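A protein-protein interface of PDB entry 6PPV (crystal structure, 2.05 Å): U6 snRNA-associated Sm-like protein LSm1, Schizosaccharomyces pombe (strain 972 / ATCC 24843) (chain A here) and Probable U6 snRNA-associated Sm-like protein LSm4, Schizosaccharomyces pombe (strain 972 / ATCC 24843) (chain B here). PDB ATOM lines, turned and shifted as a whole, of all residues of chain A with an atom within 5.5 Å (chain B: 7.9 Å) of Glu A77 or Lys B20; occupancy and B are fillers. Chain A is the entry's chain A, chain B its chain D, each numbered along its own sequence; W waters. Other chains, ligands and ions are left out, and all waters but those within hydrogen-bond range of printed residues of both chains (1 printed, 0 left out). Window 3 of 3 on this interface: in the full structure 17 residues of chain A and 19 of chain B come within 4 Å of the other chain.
Water W1 lies within hydrogen-bond range of O of Tyr B35 and NH2 of Arg A75.
NH1 of Arg A75 sits at hydrogen-bond distance from O of Tyr B35, at 3.4 Å.
NH1 of Arg A75 sits at hydrogen-bond distance from O of Gly B63.
N of Arg A75 lies within hydrogen-bond range of O of Lys B67.
The side-chain carboxylate of Glu A77 lies within salt-bridge range of the side-chain amino group of Lys B20 (2.7 Å).
The backbone carbonyl oxygen (O) of Ile B66 is in hydrogen-bond range of the side-chain amide nitrogen (ND2) of Asn A78 (3.0 Å).
The side-chain amide nitrogen of Asn A78 sits at hydrogen-bond distance from the backbone carbonyl oxygen of Lys B67 (3.2 Å).
Among the printed residues, merely in contact across the chains: Arg A31 with Lys B20, Asn A48 with Met B36, Arg A75 with Met B36, Arg A75 with Asn B64, Arg A75 with Ile B66, Glu A77 with Asn B64 and Asn A78 with Lys B20.
Of the 8 printed residues of chain A, 5 touch a printed residue of chain B.
Hydrophobic or aromatic side chains of chain B that line the printed part of chain A: Met B36.
Along chain B the printed residues that touch a printed residue of chain A span positions 20 to 67.
Among the printed residues, 13 pairs touch across the chains.
Among the printed residues, Asp or Glu carboxylates within 4 Å of a Lys or Arg side-chain nitrogen of the other chain: Glu A77 with Lys B20 (2.7 Å).
No residue of chain B comes within 4 Å of Gly A76.
Glu A77 touches just these residues of chain B: Lys B20 (2.7 Å) and Asn B64 (3.7 Å).
Printed residues of chain B within 4 Å of Asn A78: Lys B20 (3.9 Å), Ile B66 (3.0 Å) and Lys B67 (3.2 Å).
Printed residues of chain A within 4 Å of Lys B20: Arg A31, Glu A77 and Asn A78.
Asn B21 touches none of the printed residues of chain A.
Pro B48 touches none of the printed residues of chain A.
Of the printed residues of chain A, Lys B67 touches Arg A75 (3.4 Å) and Asn A78 (3.2 Å).
The nearest residue of chain B that does not touch Glu A77 is Ile B66 (4.7 Å).
The nearest residue of chain A that does not touch Lys B20 is Arg A75 (5.3 Å).
The nearest printed residue of chain A that does not touch Asn B64 is Arg A31 (6.8 Å).
The side-chain carboxylate of Glu A77 lies within salt-bridge range of the guanidinium group of Arg A31 (3.4 Å).
OE1 of Glu A77 lies within salt-bridge range of NE of Arg A75 (2.6 Å).
The side-chain carboxylate (OE1) of Glu B18 is in salt-bridge range of the side-chain amino group (NZ) of Lys B67 (2.8 Å).
The side-chain amino group of Lys B20 sits at hydrogen-bond distance from the backbone carbonyl oxygen of Asn B64 (2.7 Å).
The backbone NH (N) of Lys B20 is in hydrogen-bond range of the backbone carbonyl oxygen (O) of Asn B65.
The guanidinium group (NH1) of Arg B62 is in hydrogen-bond range of the side-chain amide oxygen (OD1) of Asn B64 (3.4 Å).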
ATOM      1  N   ARG A  31      -7.605  20.509  17.418  1.00  0.00           N
ATOM      2  CA  ARG A  31      -6.745  21.546  16.846  1.00  0.00           C
ATOM      3  C   ARG A  31      -7.298  22.082  15.540  1.00  0.00           C
ATOM      4  O   ARG A  31      -7.127  23.264  15.242  1.00  0.00           O
ATOM      5  CB  ARG A  31      -5.331  21.016  16.628  1.00  0.00           C
ATOM      6  CG  ARG A  31      -4.304  21.584  17.593  1.00  0.00           C
ATOM      7  CD  ARG A  31      -2.899  21.121  17.242  1.00  0.00           C
ATOM      8  NE  ARG A  31      -2.916  19.734  16.796  1.00  0.00           N
ATOM      9  CZ  ARG A  31      -1.835  19.000  16.555  1.00  0.00           C
ATOM     10  NH1 ARG A  31      -0.621  19.519  16.724  1.00  0.00           N
ATOM     11  NH2 ARG A  31      -1.971  17.739  16.153  1.00  0.00           N
ATOM     12  N   PHE A  46      -1.131   9.636  26.794  1.00  0.00           N
ATOM     13  CA  PHE A  46      -0.994  10.669  25.771  1.00  0.00           C
ATOM     14  C   PHE A  46      -2.204  11.576  25.709  1.00  0.00           C
ATOM     15  O   PHE A  46      -2.238  12.488  24.874  1.00  0.00           O
ATOM     16  CB  PHE A  46      -0.789  10.036  24.395  1.00  0.00           C
ATOM     17  CG  PHE A  46       0.426   9.189  24.314  1.00  0.00           C
ATOM     18  CD1 PHE A  46       1.684   9.772  24.290  1.00  0.00           C
ATOM     19  CD2 PHE A  46       0.321   7.808  24.285  1.00  0.00           C
ATOM     20  CE1 PHE A  46       2.824   8.989  24.224  1.00  0.00           C
ATOM     21  CE2 PHE A  46       1.458   7.015  24.216  1.00  0.00           C
ATOM     22  CZ  PHE A  46       2.711   7.609  24.184  1.00  0.00           C
ATOM     23  N   ASN A  48      -4.853  10.360  24.587  1.00  0.00           N
ATOM     24  CA  ASN A  48      -5.746   9.737  23.619  1.00  0.00           C
ATOM     25  C   ASN A  48      -7.094   9.539  24.295  1.00  0.00           C
ATOM     26  O   ASN A  48      -7.158   9.175  25.467  1.00  0.00           O
ATOM     27  CB  ASN A  48      -5.222   8.377  23.145  1.00  0.00           C
ATOM     28  CG  ASN A  48      -3.945   8.474  22.351  1.00  0.00           C
ATOM     29  OD1 ASN A  48      -3.724   9.441  21.617  1.00  0.00           O
ATOM     30  ND2 ASN A  48      -3.102   7.441  22.464  1.00  0.00           N
ATOM     31  N   ARG A  75      -6.672  10.935  18.771  1.00  0.00           N
ATOM     32  CA  ARG A  75      -5.255  10.975  19.123  1.00  0.00           C
ATOM     33  C   ARG A  75      -4.972  12.212  19.974  1.00  0.00           C
ATOM     34  O   ARG A  75      -5.352  13.328  19.607  1.00  0.00           O
ATOM     35  CB  ARG A  75      -4.395  10.964  17.864  1.00  0.00           C
ATOM     36  CG  ARG A  75      -2.952  10.581  18.089  1.00  0.00           C
ATOM     37  CD  ARG A  75      -2.174  10.697  16.802  1.00  0.00           C
ATOM     38  NE  ARG A  75      -0.747  10.871  17.047  1.00  0.00           N
ATOM     39  CZ  ARG A  75       0.090   9.884  17.363  1.00  0.00           C
ATOM     40  NH1 ARG A  75      -0.346   8.639  17.475  1.00  0.00           N
ATOM     41  NH2 ARG A  75       1.371  10.149  17.567  1.00  0.00           N
ATOM     42  N   GLY A  76      -4.317  12.004  21.119  1.00  0.00           N
ATOM     43  CA  GLY A  76      -4.191  13.065  22.115  1.00  0.00           C
ATOM     44  C   GLY A  76      -3.593  14.364  21.598  1.00  0.00           C
ATOM     45  O   GLY A  76      -4.018  15.453  21.993  1.00  0.00           O
ATOM     46  N   GLU A  77      -2.598  14.277  20.710  1.00  0.00           N
ATOM     47  CA  GLU A  77      -1.937  15.499  20.255  1.00  0.00           C
ATOM     48  C   GLU A  77      -2.879  16.465  19.535  1.00  0.00           C
ATOM     49  O   GLU A  77      -2.528  17.636  19.367  1.00  0.00           O
ATOM     50  CB  GLU A  77      -0.765  15.148  19.339  1.00  0.00           C
ATOM     51  CG  GLU A  77      -1.164  14.378  18.092  1.00  0.00           C
ATOM     52  CD  GLU A  77      -0.040  14.335  17.071  1.00  0.00           C
ATOM     53  OE1 GLU A  77       0.329  13.227  16.620  1.00  0.00           O
ATOM     54  OE2 GLU A  77       0.478  15.422  16.726  1.00  0.00           O
ATOM     55  N   ASN A  78      -4.057  16.016  19.119  1.00  0.00           N
ATOM     56  CA  ASN A  78      -5.012  16.866  18.425  1.00  0.00           C
ATOM     57  C   ASN A  78      -6.034  17.486  19.365  1.00  0.00           C
ATOM     58  O   ASN A  78      -6.857  18.299  18.924  1.00  0.00           O
ATOM     59  CB  ASN A  78      -5.720  16.056  17.340  1.00  0.00           C
ATOM     60  CG  ASN A  78      -4.753  15.480  16.336  1.00  0.00           C
ATOM     61  OD1 ASN A  78      -4.168  16.219  15.543  1.00  0.00           O
ATOM     62  ND2 ASN A  78      -4.558  14.162  16.371  1.00  0.00           N
ATOM     63  N   VAL A  79      -5.996  17.127  20.641  1.00  0.00           N
ATOM     64  CA  VAL A  79      -6.969  17.611  21.609  1.00  0.00           C
ATOM     65  C   VAL A  79      -6.494  18.954  22.137  1.00  0.00           C
ATOM     66  O   VAL A  79      -5.427  19.047  22.757  1.00  0.00           O
ATOM     67  CB  VAL A  79      -7.157  16.612  22.759  1.00  0.00           C
ATOM     68  CG1 VAL A  79      -7.970  17.260  23.892  1.00  0.00           C
ATOM     69  CG2 VAL A  79      -7.819  15.337  22.237  1.00  0.00           C
ATOM     70  N   VAL B  17     -10.409   6.409   9.290  1.00  0.00           N
ATOM     71  CA  VAL B  17      -9.258   7.156   9.772  1.00  0.00           C
ATOM     72  C   VAL B  17      -9.298   8.539   9.145  1.00  0.00           C
ATOM     73  O   VAL B  17      -9.351   8.663   7.918  1.00  0.00           O
ATOM     74  CB  VAL B  17      -7.938   6.449   9.418  1.00  0.00           C
ATOM     75  CG1 VAL B  17      -6.753   7.153  10.092  1.00  0.00           C
ATOM     76  CG2 VAL B  17      -8.000   5.003   9.804  1.00  0.00           C
ATOM     77  N   GLU B  18      -9.253   9.581   9.969  1.00  0.00           N
ATOM     78  CA  GLU B  18      -8.999  10.915   9.452  1.00  0.00           C
ATOM     79  C   GLU B  18      -7.588  11.351   9.821  1.00  0.00           C
ATOM     80  O   GLU B  18      -7.211  11.328  11.004  1.00  0.00           O
ATOM     81  CB  GLU B  18     -10.015  11.942   9.947  1.00  0.00           C
ATOM     82  CG  GLU B  18      -9.833  13.275   9.194  1.00  0.00           C
ATOM     83  CD  GLU B  18     -10.973  14.270   9.402  1.00  0.00           C
ATOM     84  OE1 GLU B  18     -10.691  15.487   9.470  1.00  0.00           O
ATOM     85  OE2 GLU B  18     -12.146  13.838   9.491  1.00  0.00           O
ATOM     86  N   LEU B  19      -6.825  11.750   8.802  1.00  0.00           N
ATOM     87  CA  LEU B  19      -5.475  12.283   8.944  1.00  0.00           C
ATOM     88  C   LEU B  19      -5.499  13.762   9.338  1.00  0.00           C
ATOM     89  O   LEU B  19      -6.520  14.452   9.231  1.00  0.00           O
ATOM     90  CB  LEU B  19      -4.699  12.110   7.642  1.00  0.00           C
ATOM     91  CG  LEU B  19      -4.698  10.686   7.085  1.00  0.00           C
ATOM     92  CD1 LEU B  19      -3.764  10.616   5.896  1.00  0.00           C
ATOM     93  CD2 LEU B  19      -4.282   9.691   8.178  1.00  0.00           C
ATOM     94  N   LYS B  20      -4.334  14.255   9.772  1.00  0.00           N
ATOM     95  CA  LYS B  20      -4.233  15.643  10.223  1.00  0.00           C
ATOM     96  C   LYS B  20      -4.598  16.641   9.135  1.00  0.00           C
ATOM     97  O   LYS B  20      -5.045  17.749   9.447  1.00  0.00           O
ATOM     98  CB  LYS B  20      -2.829  15.937  10.733  1.00  0.00           C
ATOM     99  CG  LYS B  20      -2.558  15.368  12.113  1.00  0.00           C
ATOM    100  CD  LYS B  20      -1.080  15.426  12.419  1.00  0.00           C
ATOM    101  CE  LYS B  20      -0.811  15.082  13.859  1.00  0.00           C
ATOM    102  NZ  LYS B  20       0.653  15.045  14.098  1.00  0.00           N
ATOM    103  N   ASN B  21      -4.424  16.286   7.864  1.00  0.00           N
ATOM    104  CA  ASN B  21      -4.760  17.208   6.788  1.00  0.00           C
ATOM    105  C   ASN B  21      -6.180  17.026   6.263  1.00  0.00           C
ATOM    106  O   ASN B  21      -6.524  17.618   5.237  1.00  0.00           O
ATOM    107  CB  ASN B  21      -3.755  17.084   5.638  1.00  0.00           C
ATOM    108  CG  ASN B  21      -3.805  15.730   4.953  1.00  0.00           C
ATOM    109  OD1 ASN B  21      -4.615  14.861   5.297  1.00  0.00           O
ATOM    110  ND2 ASN B  21      -2.941  15.546   3.968  1.00  0.00           N
ATOM    111  N   GLY B  22      -7.009  16.216   6.928  1.00  0.00           N
ATOM    112  CA  GLY B  22      -8.397  16.072   6.542  1.00  0.00           C
ATOM    113  C   GLY B  22      -8.707  14.942   5.579  1.00  0.00           C
ATOM    114  O   GLY B  22      -9.890  14.647   5.362  1.00  0.00           O
ATOM    115  N   GLU B  23      -7.699  14.308   4.983  1.00  0.00           N
ATOM    116  CA  GLU B  23      -7.933  13.076   4.234  1.00  0.00           C
ATOM    117  C   GLU B  23      -8.603  12.027   5.112  1.00  0.00           C
ATOM    118  O   GLU B  23      -8.303  11.915   6.303  1.00  0.00           O
ATOM    119  CB  GLU B  23      -6.608  12.519   3.713  1.00  0.00           C
ATOM    120  CG  GLU B  23      -6.086  13.151   2.448  1.00  0.00           C
ATOM    121  CD  GLU B  23      -4.732  12.591   2.063  1.00  0.00           C
ATOM    122  OE1 GLU B  23      -3.727  13.321   2.204  1.00  0.00           O
ATOM    123  OE2 GLU B  23      -4.671  11.411   1.650  1.00  0.00           O
ATOM    124  N   TYR B  35       2.472   2.771  18.402  1.00  0.00           N
ATOM    125  CA  TYR B  35       2.590   4.090  17.786  1.00  0.00           C
ATOM    126  C   TYR B  35       1.274   4.582  17.198  1.00  0.00           C
ATOM    127  O   TYR B  35       1.203   5.743  16.768  1.00  0.00           O
ATOM    128  CB  TYR B  35       3.616   4.080  16.649  1.00  0.00           C
ATOM    129  CG  TYR B  35       5.038   3.716  17.002  1.00  0.00           C
ATOM    130  CD1 TYR B  35       5.898   4.646  17.581  1.00  0.00           C
ATOM    131  CD2 TYR B  35       5.543   2.458  16.695  1.00  0.00           C
ATOM    132  CE1 TYR B  35       7.204   4.321  17.874  1.00  0.00           C
ATOM    133  CE2 TYR B  35       6.852   2.122  16.985  1.00  0.00           C
ATOM    134  CZ  TYR B  35       7.679   3.056  17.574  1.00  0.00           C
ATOM    135  OH  TYR B  35       8.984   2.713  17.859  1.00  0.00           O
ATOM    136  N   MET B  36       0.251   3.723  17.142  1.00  0.00           N
ATOM    137  CA  MET B  36      -0.958   3.935  16.352  1.00  0.00           C
ATOM    138  C   MET B  36      -0.691   3.857  14.848  1.00  0.00           C
ATOM    139  O   MET B  36      -1.504   4.335  14.051  1.00  0.00           O
ATOM    140  CB  MET B  36      -1.636   5.268  16.697  1.00  0.00           C
ATOM    141  CG  MET B  36      -3.101   5.163  17.028  1.00  0.00           C
ATOM    142  SD  MET B  36      -3.745   6.781  17.482  1.00  0.00           S
ATOM    143  CE  MET B  36      -2.756   7.062  18.924  1.00  0.00           C
ATOM    144  N   PRO B  48      -9.011  15.889   1.130  1.00  0.00           N
ATOM    145  CA  PRO B  48      -9.582  16.845   2.099  1.00  0.00           C
ATOM    146  C   PRO B  48     -10.840  17.561   1.627  1.00  0.00           C
ATOM    147  O   PRO B  48     -11.894  17.451   2.263  1.00  0.00           O
ATOM    148  CB  PRO B  48      -8.432  17.837   2.321  1.00  0.00           C
ATOM    149  CG  PRO B  48      -7.192  17.015   2.111  1.00  0.00           C
ATOM    150  CD  PRO B  48      -7.545  16.039   1.011  1.00  0.00           C
ATOM    151  N   ARG B  62       1.163   5.957   9.063  1.00  0.00           N
ATOM    152  CA  ARG B  62       2.026   6.214  10.201  1.00  0.00           C
ATOM    153  C   ARG B  62       1.221   6.910  11.293  1.00  0.00           C
ATOM    154  O   ARG B  62       0.450   7.832  11.024  1.00  0.00           O
ATOM    155  CB  ARG B  62       3.232   7.060   9.775  1.00  0.00           C
ATOM    156  CG  ARG B  62       4.478   6.901  10.648  1.00  0.00           C
ATOM    157  CD  ARG B  62       5.598   7.846  10.148  1.00  0.00           C
ATOM    158  NE  ARG B  62       6.963   7.405  10.455  1.00  0.00           N
ATOM    159  CZ  ARG B  62       7.672   7.870  11.480  1.00  0.00           C
ATOM    160  NH1 ARG B  62       7.148   8.789  12.284  1.00  0.00           N
ATOM    161  NH2 ARG B  62       8.906   7.430  11.696  1.00  0.00           N
ATOM    162  N   GLY B  63       1.419   6.469  12.537  1.00  0.00           N
ATOM    163  CA  GLY B  63       0.540   6.895  13.624  1.00  0.00           C
ATOM    164  C   GLY B  63       0.510   8.398  13.866  1.00  0.00           C
ATOM    165  O   GLY B  63      -0.532   8.953  14.223  1.00  0.00           O
ATOM    166  N   ASN B  64       1.648   9.080  13.692  1.00  0.00           N
ATOM    167  CA  ASN B  64       1.680  10.493  14.062  1.00  0.00           C
ATOM    168  C   ASN B  64       1.107  11.395  12.979  1.00  0.00           C
ATOM    169  O   ASN B  64       1.232  12.619  13.070  1.00  0.00           O
ATOM    170  CB  ASN B  64       3.106  10.931  14.448  1.00  0.00           C
ATOM    171  CG  ASN B  64       4.076  10.924  13.291  1.00  0.00           C
ATOM    172  OD1 ASN B  64       3.999  10.093  12.380  1.00  0.00           O
ATOM    173  ND2 ASN B  64       5.017  11.856  13.327  1.00  0.00           N
ATOM    174  N   ASN B  65       0.470  10.812  11.969  1.00  0.00           N
ATOM    175  CA  ASN B  65      -0.286  11.552  10.969  1.00  0.00           C
ATOM    176  C   ASN B  65      -1.796  11.519  11.229  1.00  0.00           C
ATOM    177  O   ASN B  65      -2.556  12.150  10.485  1.00  0.00           O
ATOM    178  CB  ASN B  65       0.030  10.986   9.571  1.00  0.00           C
ATOM    179  CG  ASN B  65      -0.457  11.884   8.441  1.00  0.00           C
ATOM    180  OD1 ASN B  65      -0.552  13.101   8.598  1.00  0.00           O
ATOM    181  ND2 ASN B  65      -0.775  11.280   7.293  1.00  0.00           N
ATOM    182  N   ILE B  66      -2.252  10.821  12.275  1.00  0.00           N
ATOM    183  CA  ILE B  66      -3.684  10.609  12.499  1.00  0.00           C
ATOM    184  C   ILE B  66      -4.276  11.761  13.309  1.00  0.00           C
ATOM    185  O   ILE B  66      -3.690  12.224  14.297  1.00  0.00           O
ATOM    186  CB  ILE B  66      -3.924   9.254  13.191  1.00  0.00           C
ATOM    187  CG1 ILE B  66      -3.598   8.104  12.225  1.00  0.00           C
ATOM    188  CG2 ILE B  66      -5.374   9.132  13.718  1.00  0.00           C
ATOM    189  CD1 ILE B  66      -3.506   6.747  12.907  1.00  0.00           C
ATOM    190  N   LYS B  67      -5.438  12.241  12.867  1.00  0.00           N
ATOM    191  CA  LYS B  67      -6.291  13.114  13.667  1.00  0.00           C
ATOM    192  C   LYS B  67      -7.228  12.297  14.562  1.00  0.00           C
ATOM    193  O   LYS B  67      -7.180  12.408  15.793  1.00  0.00           O
ATOM    194  CB  LYS B  67      -7.095  14.047  12.752  1.00  0.00           C
ATOM    195  CG  LYS B  67      -8.039  14.995  13.508  1.00  0.00           C
ATOM    196  CD  LYS B  67      -8.898  15.816  12.546  1.00  0.00           C
ATOM    197  CE  LYS B  67      -8.026  16.555  11.528  1.00  0.00           C
ATOM    198  NZ  LYS B  67      -8.853  17.338  10.575  1.00  0.00           N
ATOM    199  N   TYR B  68      -8.067  11.453  13.965  1.00  0.00           N
ATOM    200  CA  TYR B  68      -8.875  10.569  14.801  1.00  0.00           C
ATOM    201  C   TYR B  68      -9.284   9.327  14.029  1.00  0.00           C
ATOM    202  O   TYR B  68      -9.039   9.192  12.830  1.00  0.00           O
ATOM    203  CB  TYR B  68     -10.133  11.262  15.368  1.00  0.00           C
ATOM    204  CG  TYR B  68     -11.014  11.906  14.328  1.00  0.00           C
ATOM    205  CD1 TYR B  68     -11.783  11.137  13.458  1.00  0.00           C
ATOM    206  CD2 TYR B  68     -11.081  13.285  14.210  1.00  0.00           C
ATOM    207  CE1 TYR B  68     -12.578  11.727  12.487  1.00  0.00           C
ATOM    208  CE2 TYR B  68     -11.873  13.882  13.244  1.00  0.00           C
ATOM    209  CZ  TYR B  68     -12.616  13.096  12.390  1.00  0.00           C
ATOM    210  OH  TYR B  68     -13.406  13.683  11.436  1.00  0.00           O
HETATM  211  O   HOH W   1       3.057   7.739  17.788  1.00  0.00           O
